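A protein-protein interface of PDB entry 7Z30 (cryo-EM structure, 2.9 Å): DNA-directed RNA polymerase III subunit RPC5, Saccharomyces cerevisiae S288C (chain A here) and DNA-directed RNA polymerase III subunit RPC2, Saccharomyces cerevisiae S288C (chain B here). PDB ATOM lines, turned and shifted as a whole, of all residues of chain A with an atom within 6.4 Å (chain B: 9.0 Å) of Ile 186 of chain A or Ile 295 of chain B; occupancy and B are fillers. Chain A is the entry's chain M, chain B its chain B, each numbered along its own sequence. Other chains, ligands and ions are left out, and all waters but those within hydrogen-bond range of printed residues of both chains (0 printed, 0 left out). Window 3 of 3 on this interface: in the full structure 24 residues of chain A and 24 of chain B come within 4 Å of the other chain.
The backbone carbonyl oxygen (O) of Ile 186 of chain A lies close to the side-chain amide oxygen (OD1) of Asn 190 of chain A (2.9 Å).
The side-chain carboxylate (OD2) of Asp 294 of chain B lies within hydrogen-bond range of the side-chain amide nitrogen (NE2) of Gln 300 of chain B.
The backbone carbonyl oxygen (O) of Ile 295 of chain B sits close to the side-chain amide oxygen (OE1) of Gln 300 of chain B (2.7 Å).
The side-chain hydroxyl of Thr 297 of chain B lies within hydrogen-bond range of the backbone NH of Gln 299 of chain B, at 3.3 Å.
N of Gln 300 of chain B sits at hydrogen-bond distance from OG1 of Thr 297 of chain B (3.2 Å).
Among the printed residues, merely in contact across the chains: Phe 183 of chain A with Thr 297 of chain B (3.5 Å), Asn 190 of chain A with Gln 300 of chain B (3.6 Å), Ile 186 of chain A with Thr 297 of chain B (3.7 Å), Ile 186 of chain A with Ile 295 of chain B (3.7 Å) and Ile 186 of chain A with Gln 300 of chain B (3.8 Å).
The side-chain amide oxygen (OE1) of Gln 299 of chain B sits close to the side-chain carboxylate (OD2) of Asp 187 of chain A, 2.7 Å away.
Ile 186 of chain A touches three residues of chain B.
Of the printed residues of chain B, Asn 190 of chain A touches Gln 300.
Leu 263 of chain B touches none of the printed residues of chain A.
Ser 290 of chain B touches none of the printed residues of chain A.
Of chain A, only Ile 186 comes within 4 Å of Ile 295 of chain B.
Of the printed residues of chain A, Gln 299 of chain B touches Asp 187 (2.7 Å).
The nearest residue of chain B that does not touch Ile 186 of chain A is Tyr 296 of chain B (5.7 Å).
The nearest residue of chain A that does not touch Ile 295 of chain B is Trp 140 of chain A (5.4 Å).
The nearest printed residue of chain B that does not touch Asp 187 of chain A is Thr 297 of chain B (4.9 Å).
Of the 10 printed residues of chain A, 4 touch a printed residue of chain B.
Printed residues of chain A that touch a printed residue of chain B: Phe 183, Ile 186, Asp 187 and Asn 190.
Among the printed residues, 6 pairs touch across the chains.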
ATOM      1  N   TRP A 140      -4.955 -35.364 -14.986  1.00  0.00           N
ATOM      2  CA  TRP A 140      -4.285 -35.831 -16.195  1.00  0.00           C
ATOM      3  C   TRP A 140      -3.489 -37.087 -15.873  1.00  0.00           C
ATOM      4  O   TRP A 140      -2.892 -37.186 -14.799  1.00  0.00           O
ATOM      5  CB  TRP A 140      -3.366 -34.746 -16.768  1.00  0.00           C
ATOM      6  CG  TRP A 140      -4.012 -33.395 -16.857  1.00  0.00           C
ATOM      7  CD1 TRP A 140      -4.979 -33.003 -17.738  1.00  0.00           C
ATOM      8  CD2 TRP A 140      -3.745 -32.260 -16.025  1.00  0.00           C
ATOM      9  NE1 TRP A 140      -5.327 -31.695 -17.508  1.00  0.00           N
ATOM     10  CE2 TRP A 140      -4.584 -31.215 -16.460  1.00  0.00           C
ATOM     11  CE3 TRP A 140      -2.876 -32.025 -14.955  1.00  0.00           C
ATOM     12  CZ2 TRP A 140      -4.578 -29.955 -15.865  1.00  0.00           C
ATOM     13  CZ3 TRP A 140      -2.872 -30.772 -14.366  1.00  0.00           C
ATOM     14  CH2 TRP A 140      -3.717 -29.755 -14.821  1.00  0.00           C
ATOM     15  N   PHE A 183       1.344 -28.421 -22.766  1.00  0.00           N
ATOM     16  CA  PHE A 183       0.400 -29.192 -21.966  1.00  0.00           C
ATOM     17  C   PHE A 183      -0.301 -30.272 -22.788  1.00  0.00           C
ATOM     18  O   PHE A 183      -1.527 -30.240 -22.961  1.00  0.00           O
ATOM     19  CB  PHE A 183      -0.613 -28.245 -21.327  1.00  0.00           C
ATOM     20  CG  PHE A 183       0.022 -27.084 -20.617  1.00  0.00           C
ATOM     21  CD1 PHE A 183       0.748 -27.281 -19.459  1.00  0.00           C
ATOM     22  CD2 PHE A 183      -0.087 -25.798 -21.119  1.00  0.00           C
ATOM     23  CE1 PHE A 183       1.343 -26.219 -18.805  1.00  0.00           C
ATOM     24  CE2 PHE A 183       0.506 -24.732 -20.467  1.00  0.00           C
ATOM     25  CZ  PHE A 183       1.221 -24.944 -19.309  1.00  0.00           C
ATOM     26  N   LYS A 184       0.471 -31.242 -23.292  1.00  0.00           N
ATOM     27  CA  LYS A 184      -0.107 -32.317 -24.093  1.00  0.00           C
ATOM     28  C   LYS A 184      -1.083 -33.165 -23.286  1.00  0.00           C
ATOM     29  O   LYS A 184      -2.028 -33.733 -23.846  1.00  0.00           O
ATOM     30  CB  LYS A 184       1.005 -33.190 -24.675  1.00  0.00           C
ATOM     31  CG  LYS A 184       2.310 -33.134 -23.894  1.00  0.00           C
ATOM     32  CD  LYS A 184       3.348 -34.082 -24.473  1.00  0.00           C
ATOM     33  CE  LYS A 184       3.817 -33.617 -25.841  1.00  0.00           C
ATOM     34  NZ  LYS A 184       4.635 -34.650 -26.533  1.00  0.00           N
ATOM     35  N   TYR A 185      -0.874 -33.265 -21.973  1.00  0.00           N
ATOM     36  CA  TYR A 185      -1.828 -33.988 -21.140  1.00  0.00           C
ATOM     37  C   TYR A 185      -3.157 -33.246 -21.044  1.00  0.00           C
ATOM     38  O   TYR A 185      -4.225 -33.872 -21.030  1.00  0.00           O
ATOM     39  CB  TYR A 185      -1.211 -34.274 -19.767  1.00  0.00           C
ATOM     40  CG  TYR A 185      -0.675 -33.080 -18.996  1.00  0.00           C
ATOM     41  CD1 TYR A 185      -1.513 -32.082 -18.524  1.00  0.00           C
ATOM     42  CD2 TYR A 185       0.683 -32.966 -18.735  1.00  0.00           C
ATOM     43  CE1 TYR A 185      -1.015 -31.004 -17.819  1.00  0.00           C
ATOM     44  CE2 TYR A 185       1.189 -31.893 -18.032  1.00  0.00           C
ATOM     45  CZ  TYR A 185       0.336 -30.915 -17.575  1.00  0.00           C
ATOM     46  OH  TYR A 185       0.836 -29.843 -16.874  1.00  0.00           O
ATOM     47  N   ILE A 186      -3.117 -31.913 -21.017  1.00  0.00           N
ATOM     48  CA  ILE A 186      -4.349 -31.135 -21.114  1.00  0.00           C
ATOM     49  C   ILE A 186      -4.996 -31.353 -22.474  1.00  0.00           C
ATOM     50  O   ILE A 186      -6.223 -31.480 -22.582  1.00  0.00           O
ATOM     51  CB  ILE A 186      -4.074 -29.645 -20.842  1.00  0.00           C
ATOM     52  CG1 ILE A 186      -3.830 -29.416 -19.351  1.00  0.00           C
ATOM     53  CG2 ILE A 186      -5.239 -28.793 -21.301  1.00  0.00           C
ATOM     54  CD1 ILE A 186      -3.811 -27.964 -18.974  1.00  0.00           C
ATOM     55  N   ASP A 187      -4.179 -31.407 -23.532  1.00  0.00           N
ATOM     56  CA  ASP A 187      -4.693 -31.740 -24.862  1.00  0.00           C
ATOM     57  C   ASP A 187      -5.484 -33.043 -24.840  1.00  0.00           C
ATOM     58  O   ASP A 187      -6.614 -33.115 -25.343  1.00  0.00           O
ATOM     59  CB  ASP A 187      -3.540 -31.863 -25.860  1.00  0.00           C
ATOM     60  CG  ASP A 187      -3.990 -31.755 -27.295  1.00  0.00           C
ATOM     61  OD1 ASP A 187      -5.196 -31.948 -27.580  1.00  0.00           O
ATOM     62  OD2 ASP A 187      -3.126 -31.519 -28.173  1.00  0.00           O
ATOM     63  N   ASP A 188      -4.886 -34.094 -24.283  1.00  0.00           N
ATOM     64  CA  ASP A 188      -5.505 -35.413 -24.334  1.00  0.00           C
ATOM     65  C   ASP A 188      -6.729 -35.491 -23.427  1.00  0.00           C
ATOM     66  O   ASP A 188      -7.728 -36.126 -23.783  1.00  0.00           O
ATOM     67  CB  ASP A 188      -4.476 -36.484 -23.976  1.00  0.00           C
ATOM     68  CG  ASP A 188      -3.496 -36.741 -25.107  1.00  0.00           C
ATOM     69  OD1 ASP A 188      -3.556 -36.014 -26.122  1.00  0.00           O
ATOM     70  OD2 ASP A 188      -2.667 -37.668 -24.984  1.00  0.00           O
ATOM     71  N   ALA A 189      -6.679 -34.848 -22.258  1.00  0.00           N
ATOM     72  CA  ALA A 189      -7.863 -34.786 -21.408  1.00  0.00           C
ATOM     73  C   ALA A 189      -9.004 -34.069 -22.116  1.00  0.00           C
ATOM     74  O   ALA A 189     -10.157 -34.517 -22.066  1.00  0.00           O
ATOM     75  CB  ALA A 189      -7.526 -34.092 -20.089  1.00  0.00           C
ATOM     76  N   ASN A 190      -8.700 -32.964 -22.802  1.00  0.00           N
ATOM     77  CA  ASN A 190      -9.731 -32.241 -23.539  1.00  0.00           C
ATOM     78  C   ASN A 190     -10.309 -33.086 -24.664  1.00  0.00           C
ATOM     79  O   ASN A 190     -11.525 -33.075 -24.888  1.00  0.00           O
ATOM     80  CB  ASN A 190      -9.163 -30.934 -24.092  1.00  0.00           C
ATOM     81  CG  ASN A 190      -8.960 -29.886 -23.018  1.00  0.00           C
ATOM     82  OD1 ASN A 190      -7.953 -29.180 -23.006  1.00  0.00           O
ATOM     83  ND2 ASN A 190      -9.923 -29.773 -22.110  1.00  0.00           N
ATOM     84  N   VAL A 191      -9.462 -33.815 -25.396  1.00  0.00           N
ATOM     85  CA  VAL A 191      -9.980 -34.611 -26.506  1.00  0.00           C
ATOM     86  C   VAL A 191     -10.820 -35.777 -25.985  1.00  0.00           C
ATOM     87  O   VAL A 191     -11.849 -36.128 -26.578  1.00  0.00           O
ATOM     88  CB  VAL A 191      -8.841 -35.075 -27.439  1.00  0.00           C
ATOM     89  CG1 VAL A 191      -8.049 -36.224 -26.843  1.00  0.00           C
ATOM     90  CG2 VAL A 191      -9.402 -35.464 -28.802  1.00  0.00           C
ATOM     91  N   ILE B 255      -6.285 -14.303 -24.750  1.00  0.00           N
ATOM     92  CA  ILE B 255      -6.634 -15.477 -25.545  1.00  0.00           C
ATOM     93  C   ILE B 255      -5.886 -15.463 -26.873  1.00  0.00           C
ATOM     94  O   ILE B 255      -5.270 -16.458 -27.267  1.00  0.00           O
ATOM     95  CB  ILE B 255      -8.159 -15.549 -25.754  1.00  0.00           C
ATOM     96  CG1 ILE B 255      -8.912 -15.247 -24.453  1.00  0.00           C
ATOM     97  CG2 ILE B 255      -8.562 -16.911 -26.294  1.00  0.00           C
ATOM     98  CD1 ILE B 255      -8.420 -16.016 -23.244  1.00  0.00           C
ATOM     99  N   LYS B 258      -2.110 -15.940 -26.337  1.00  0.00           N
ATOM    100  CA  LYS B 258      -1.775 -17.343 -26.114  1.00  0.00           C
ATOM    101  C   LYS B 258      -1.915 -18.151 -27.397  1.00  0.00           C
ATOM    102  O   LYS B 258      -1.128 -19.070 -27.647  1.00  0.00           O
ATOM    103  CB  LYS B 258      -2.653 -17.920 -25.007  1.00  0.00           C
ATOM    104  CG  LYS B 258      -2.065 -17.744 -23.618  1.00  0.00           C
ATOM    105  CD  LYS B 258      -2.889 -18.448 -22.560  1.00  0.00           C
ATOM    106  CE  LYS B 258      -2.171 -18.445 -21.220  1.00  0.00           C
ATOM    107  NZ  LYS B 258      -0.917 -19.247 -21.251  1.00  0.00           N
ATOM    108  N   LEU B 263       2.339 -18.423 -25.149  1.00  0.00           N
ATOM    109  CA  LEU B 263       1.386 -19.102 -24.277  1.00  0.00           C
ATOM    110  C   LEU B 263       1.891 -19.251 -22.845  1.00  0.00           C
ATOM    111  O   LEU B 263       1.359 -20.074 -22.094  1.00  0.00           O
ATOM    112  CB  LEU B 263       1.031 -20.471 -24.865  1.00  0.00           C
ATOM    113  CG  LEU B 263       2.176 -21.481 -24.986  1.00  0.00           C
ATOM    114  CD1 LEU B 263       2.119 -22.522 -23.879  1.00  0.00           C
ATOM    115  CD2 LEU B 263       2.182 -22.147 -26.357  1.00  0.00           C
ATOM    116  N   SER B 264       2.880 -18.457 -22.432  1.00  0.00           N
ATOM    117  CA  SER B 264       3.489 -18.682 -21.124  1.00  0.00           C
ATOM    118  C   SER B 264       2.833 -17.847 -20.029  1.00  0.00           C
ATOM    119  O   SER B 264       2.980 -18.168 -18.845  1.00  0.00           O
ATOM    120  CB  SER B 264       4.988 -18.391 -21.186  1.00  0.00           C
ATOM    121  OG  SER B 264       5.435 -17.758 -20.001  1.00  0.00           O
ATOM    122  N   ASP B 265       2.134 -16.772 -20.400  1.00  0.00           N
ATOM    123  CA  ASP B 265       1.343 -15.941 -19.489  1.00  0.00           C
ATOM    124  C   ASP B 265       2.191 -15.157 -18.491  1.00  0.00           C
ATOM    125  O   ASP B 265       1.651 -14.412 -17.669  1.00  0.00           O
ATOM    126  CB  ASP B 265       0.313 -16.787 -18.739  1.00  0.00           C
ATOM    127  CG  ASP B 265      -0.872 -15.975 -18.252  1.00  0.00           C
ATOM    128  OD1 ASP B 265      -1.764 -15.664 -19.069  1.00  0.00           O
ATOM    129  OD2 ASP B 265      -0.909 -15.646 -17.049  1.00  0.00           O
ATOM    130  N   LEU B 287      -5.085 -10.749 -17.818  1.00  0.00           N
ATOM    131  CA  LEU B 287      -4.315 -11.937 -17.470  1.00  0.00           C
ATOM    132  C   LEU B 287      -5.148 -12.893 -16.623  1.00  0.00           C
ATOM    133  O   LEU B 287      -5.141 -14.107 -16.854  1.00  0.00           O
ATOM    134  CB  LEU B 287      -3.041 -11.536 -16.729  1.00  0.00           C
ATOM    135  CG  LEU B 287      -1.729 -12.138 -17.224  1.00  0.00           C
ATOM    136  CD1 LEU B 287      -1.531 -11.823 -18.689  1.00  0.00           C
ATOM    137  CD2 LEU B 287      -0.568 -11.605 -16.403  1.00  0.00           C
ATOM    138  N   GLU B 288      -5.870 -12.347 -15.643  1.00  0.00           N
ATOM    139  CA  GLU B 288      -6.738 -13.159 -14.793  1.00  0.00           C
ATOM    140  C   GLU B 288      -7.845 -13.828 -15.598  1.00  0.00           C
ATOM    141  O   GLU B 288      -8.169 -15.004 -15.377  1.00  0.00           O
ATOM    142  CB  GLU B 288      -7.341 -12.285 -13.699  1.00  0.00           C
ATOM    143  CG  GLU B 288      -6.548 -12.244 -12.418  1.00  0.00           C
ATOM    144  CD  GLU B 288      -7.058 -11.175 -11.485  1.00  0.00           C
ATOM    145  OE1 GLU B 288      -8.109 -11.404 -10.859  1.00  0.00           O
ATOM    146  OE2 GLU B 288      -6.407 -10.114 -11.374  1.00  0.00           O
ATOM    147  N   GLU B 289      -8.450 -13.087 -16.529  1.00  0.00           N
ATOM    148  CA  GLU B 289      -9.509 -13.664 -17.351  1.00  0.00           C
ATOM    149  C   GLU B 289      -9.047 -14.903 -18.105  1.00  0.00           C
ATOM    150  O   GLU B 289      -9.867 -15.794 -18.350  1.00  0.00           O
ATOM    151  CB  GLU B 289     -10.051 -12.602 -18.323  1.00  0.00           C
ATOM    152  CG  GLU B 289      -9.192 -12.353 -19.562  1.00  0.00           C
ATOM    153  CD  GLU B 289      -9.367 -13.343 -20.715  1.00  0.00           C
ATOM    154  OE1 GLU B 289     -10.035 -14.385 -20.569  1.00  0.00           O
ATOM    155  OE2 GLU B 289      -8.740 -13.106 -21.761  1.00  0.00           O
ATOM    156  N   SER B 290      -7.764 -14.987 -18.464  1.00  0.00           N
ATOM    157  CA  SER B 290      -7.295 -16.109 -19.272  1.00  0.00           C
ATOM    158  C   SER B 290      -7.497 -17.430 -18.544  1.00  0.00           C
ATOM    159  O   SER B 290      -7.843 -18.442 -19.163  1.00  0.00           O
ATOM    160  CB  SER B 290      -5.827 -15.908 -19.644  1.00  0.00           C
ATOM    161  OG  SER B 290      -5.002 -15.944 -18.495  1.00  0.00           O
ATOM    162  N   SER B 291      -7.291 -17.439 -17.231  1.00  0.00           N
ATOM    163  CA  SER B 291      -7.623 -18.600 -16.423  1.00  0.00           C
ATOM    164  C   SER B 291      -9.071 -18.601 -15.956  1.00  0.00           C
ATOM    165  O   SER B 291      -9.585 -19.664 -15.592  1.00  0.00           O
ATOM    166  CB  SER B 291      -6.705 -18.679 -15.202  1.00  0.00           C
ATOM    167  OG  SER B 291      -7.367 -19.323 -14.132  1.00  0.00           O
ATOM    168  N   LYS B 292      -9.730 -17.438 -15.950  1.00  0.00           N
ATOM    169  CA  LYS B 292     -11.125 -17.373 -15.516  1.00  0.00           C
ATOM    170  C   LYS B 292     -12.013 -18.317 -16.317  1.00  0.00           C
ATOM    171  O   LYS B 292     -12.901 -18.970 -15.754  1.00  0.00           O
ATOM    172  CB  LYS B 292     -11.642 -15.941 -15.634  1.00  0.00           C
ATOM    173  CG  LYS B 292     -12.992 -15.706 -14.985  1.00  0.00           C
ATOM    174  CD  LYS B 292     -12.839 -14.982 -13.661  1.00  0.00           C
ATOM    175  CE  LYS B 292     -11.896 -13.798 -13.781  1.00  0.00           C
ATOM    176  NZ  LYS B 292     -11.879 -12.979 -12.539  1.00  0.00           N
ATOM    177  N   LEU B 293     -11.793 -18.406 -17.628  1.00  0.00           N
ATOM    178  CA  LEU B 293     -12.643 -19.248 -18.464  1.00  0.00           C
ATOM    179  C   LEU B 293     -12.254 -20.715 -18.326  1.00  0.00           C
ATOM    180  O   LEU B 293     -13.051 -21.547 -17.878  1.00  0.00           O
ATOM    181  CB  LEU B 293     -12.549 -18.791 -19.920  1.00  0.00           C
ATOM    182  CG  LEU B 293     -12.678 -17.281 -20.140  1.00  0.00           C
ATOM    183  CD1 LEU B 293     -12.616 -16.939 -21.615  1.00  0.00           C
ATOM    184  CD2 LEU B 293     -13.966 -16.756 -19.527  1.00  0.00           C
ATOM    185  N   ASP B 294     -11.023 -21.043 -18.704  1.00  0.00           N
ATOM    186  CA  ASP B 294     -10.415 -22.350 -18.485  1.00  0.00           C
ATOM    187  C   ASP B 294      -8.949 -22.230 -18.861  1.00  0.00           C
ATOM    188  O   ASP B 294      -8.596 -21.536 -19.819  1.00  0.00           O
ATOM    189  CB  ASP B 294     -11.097 -23.460 -19.295  1.00  0.00           C
ATOM    190  CG  ASP B 294     -11.424 -23.038 -20.713  1.00  0.00           C
ATOM    191  OD1 ASP B 294     -11.337 -21.829 -21.011  1.00  0.00           O
ATOM    192  OD2 ASP B 294     -11.761 -23.919 -21.532  1.00  0.00           O
ATOM    193  N   ILE B 295      -8.095 -22.907 -18.086  1.00  0.00           N
ATOM    194  CA  ILE B 295      -6.662 -22.795 -18.334  1.00  0.00           C
ATOM    195  C   ILE B 295      -6.343 -23.286 -19.741  1.00  0.00           C
ATOM    196  O   ILE B 295      -6.972 -24.206 -20.277  1.00  0.00           O
ATOM    197  CB  ILE B 295      -5.838 -23.541 -17.271  1.00  0.00           C
ATOM    198  CG1 ILE B 295      -4.497 -22.834 -17.095  1.00  0.00           C
ATOM    199  CG2 ILE B 295      -5.656 -25.011 -17.631  1.00  0.00           C
ATOM    200  CD1 ILE B 295      -4.650 -21.408 -16.615  1.00  0.00           C
ATOM    201  N   TYR B 296      -5.369 -22.630 -20.364  1.00  0.00           N
ATOM    202  CA  TYR B 296      -5.237 -22.671 -21.810  1.00  0.00           C
ATOM    203  C   TYR B 296      -3.882 -23.195 -22.246  1.00  0.00           C
ATOM    204  O   TYR B 296      -2.844 -22.832 -21.682  1.00  0.00           O
ATOM    205  CB  TYR B 296      -5.454 -21.284 -22.408  1.00  0.00           C
ATOM    206  CG  TYR B 296      -6.907 -20.938 -22.586  1.00  0.00           C
ATOM    207  CD1 TYR B 296      -7.818 -21.898 -22.996  1.00  0.00           C
ATOM    208  CD2 TYR B 296      -7.370 -19.659 -22.335  1.00  0.00           C
ATOM    209  CE1 TYR B 296      -9.149 -21.591 -23.160  1.00  0.00           C
ATOM    210  CE2 TYR B 296      -8.698 -19.343 -22.492  1.00  0.00           C
ATOM    211  CZ  TYR B 296      -9.582 -20.310 -22.907  1.00  0.00           C
ATOM    212  OH  TYR B 296     -10.911 -19.996 -23.062  1.00  0.00           O
ATOM    213  N   THR B 297      -3.912 -24.058 -23.255  1.00  0.00           N
ATOM    214  CA  THR B 297      -2.775 -24.322 -24.114  1.00  0.00           C
ATOM    215  C   THR B 297      -2.883 -23.408 -25.327  1.00  0.00           C
ATOM    216  O   THR B 297      -3.809 -22.604 -25.444  1.00  0.00           O
ATOM    217  CB  THR B 297      -2.743 -25.785 -24.545  1.00  0.00           C
ATOM    218  OG1 THR B 297      -3.775 -26.015 -25.513  1.00  0.00           O
ATOM    219  CG2 THR B 297      -2.986 -26.683 -23.356  1.00  0.00           C
ATOM    220  N   GLN B 298      -1.933 -23.527 -26.252  1.00  0.00           N
ATOM    221  CA  GLN B 298      -2.046 -22.762 -27.487  1.00  0.00           C
ATOM    222  C   GLN B 298      -3.272 -23.197 -28.281  1.00  0.00           C
ATOM    223  O   GLN B 298      -4.067 -22.359 -28.726  1.00  0.00           O
ATOM    224  CB  GLN B 298      -0.773 -22.908 -28.317  1.00  0.00           C
ATOM    225  CG  GLN B 298      -0.952 -22.552 -29.776  1.00  0.00           C
ATOM    226  CD  GLN B 298       0.351 -22.202 -30.460  1.00  0.00           C
ATOM    227  OE1 GLN B 298       1.395 -22.102 -29.819  1.00  0.00           O
ATOM    228  NE2 GLN B 298       0.300 -22.038 -31.776  1.00  0.00           N
ATOM    229  N   GLN B 299      -3.470 -24.512 -28.426  1.00  0.00           N
ATOM    230  CA  GLN B 299      -4.542 -25.007 -29.285  1.00  0.00           C
ATOM    231  C   GLN B 299      -5.915 -24.776 -28.671  1.00  0.00           C
ATOM    232  O   GLN B 299      -6.904 -24.667 -29.402  1.00  0.00           O
ATOM    233  CB  GLN B 299      -4.339 -26.485 -29.594  1.00  0.00           C
ATOM    234  CG  GLN B 299      -5.111 -27.406 -28.699  1.00  0.00           C
ATOM    235  CD  GLN B 299      -4.446 -28.740 -28.568  1.00  0.00           C
ATOM    236  OE1 GLN B 299      -3.509 -28.893 -27.794  1.00  0.00           O
ATOM    237  NE2 GLN B 299      -4.905 -29.711 -29.341  1.00  0.00           N
ATOM    238  N   GLN B 300      -6.003 -24.687 -27.344  1.00  0.00           N
ATOM    239  CA  GLN B 300      -7.280 -24.360 -26.723  1.00  0.00           C
ATOM    240  C   GLN B 300      -7.711 -22.951 -27.108  1.00  0.00           C
ATOM    241  O   GLN B 300      -8.862 -22.719 -27.506  1.00  0.00           O
ATOM    242  CB  GLN B 300      -7.167 -24.525 -25.208  1.00  0.00           C
ATOM    243  CG  GLN B 300      -8.168 -25.503 -24.618  1.00  0.00           C
ATOM    244  CD  GLN B 300      -8.095 -25.553 -23.110  1.00  0.00           C
ATOM    245  OE1 GLN B 300      -7.012 -25.673 -22.540  1.00  0.00           O
ATOM    246  NE2 GLN B 300      -9.245 -25.458 -22.452  1.00  0.00           N
ATOM    247  N   ALA B 301      -6.776 -22.000 -27.043  1.00  0.00           N
ATOM    248  CA  ALA B 301      -7.047 -20.651 -27.524  1.00  0.00           C
ATOM    249  C   ALA B 301      -7.328 -20.632 -29.022  1.00  0.00           C
ATOM    250  O   ALA B 301      -8.178 -19.859 -29.481  1.00  0.00           O
ATOM    251  CB  ALA B 301      -5.870 -19.735 -27.196  1.00  0.00           C
ATOM    252  N   GLU B 303      -8.757 -23.007 -30.819  1.00  0.00           N
ATOM    253  CA  GLU B 303     -10.136 -23.461 -30.978  1.00  0.00           C
ATOM    254  C   GLU B 303     -11.122 -22.386 -30.548  1.00  0.00           C
ATOM    255  O   GLU B 303     -12.173 -22.203 -31.181  1.00  0.00           O
ATOM    256  CB  GLU B 303     -10.381 -24.740 -30.177  1.00  0.00           C
ATOM    257  CG  GLU B 303      -9.639 -25.959 -30.668  1.00  0.00           C
ATOM    258  CD  GLU B 303      -9.921 -27.176 -29.814  1.00  0.00           C
ATOM    259  OE1 GLU B 303     -10.831 -27.101 -28.962  1.00  0.00           O
ATOM    260  OE2 GLU B 303      -9.245 -28.209 -30.000  1.00  0.00           O
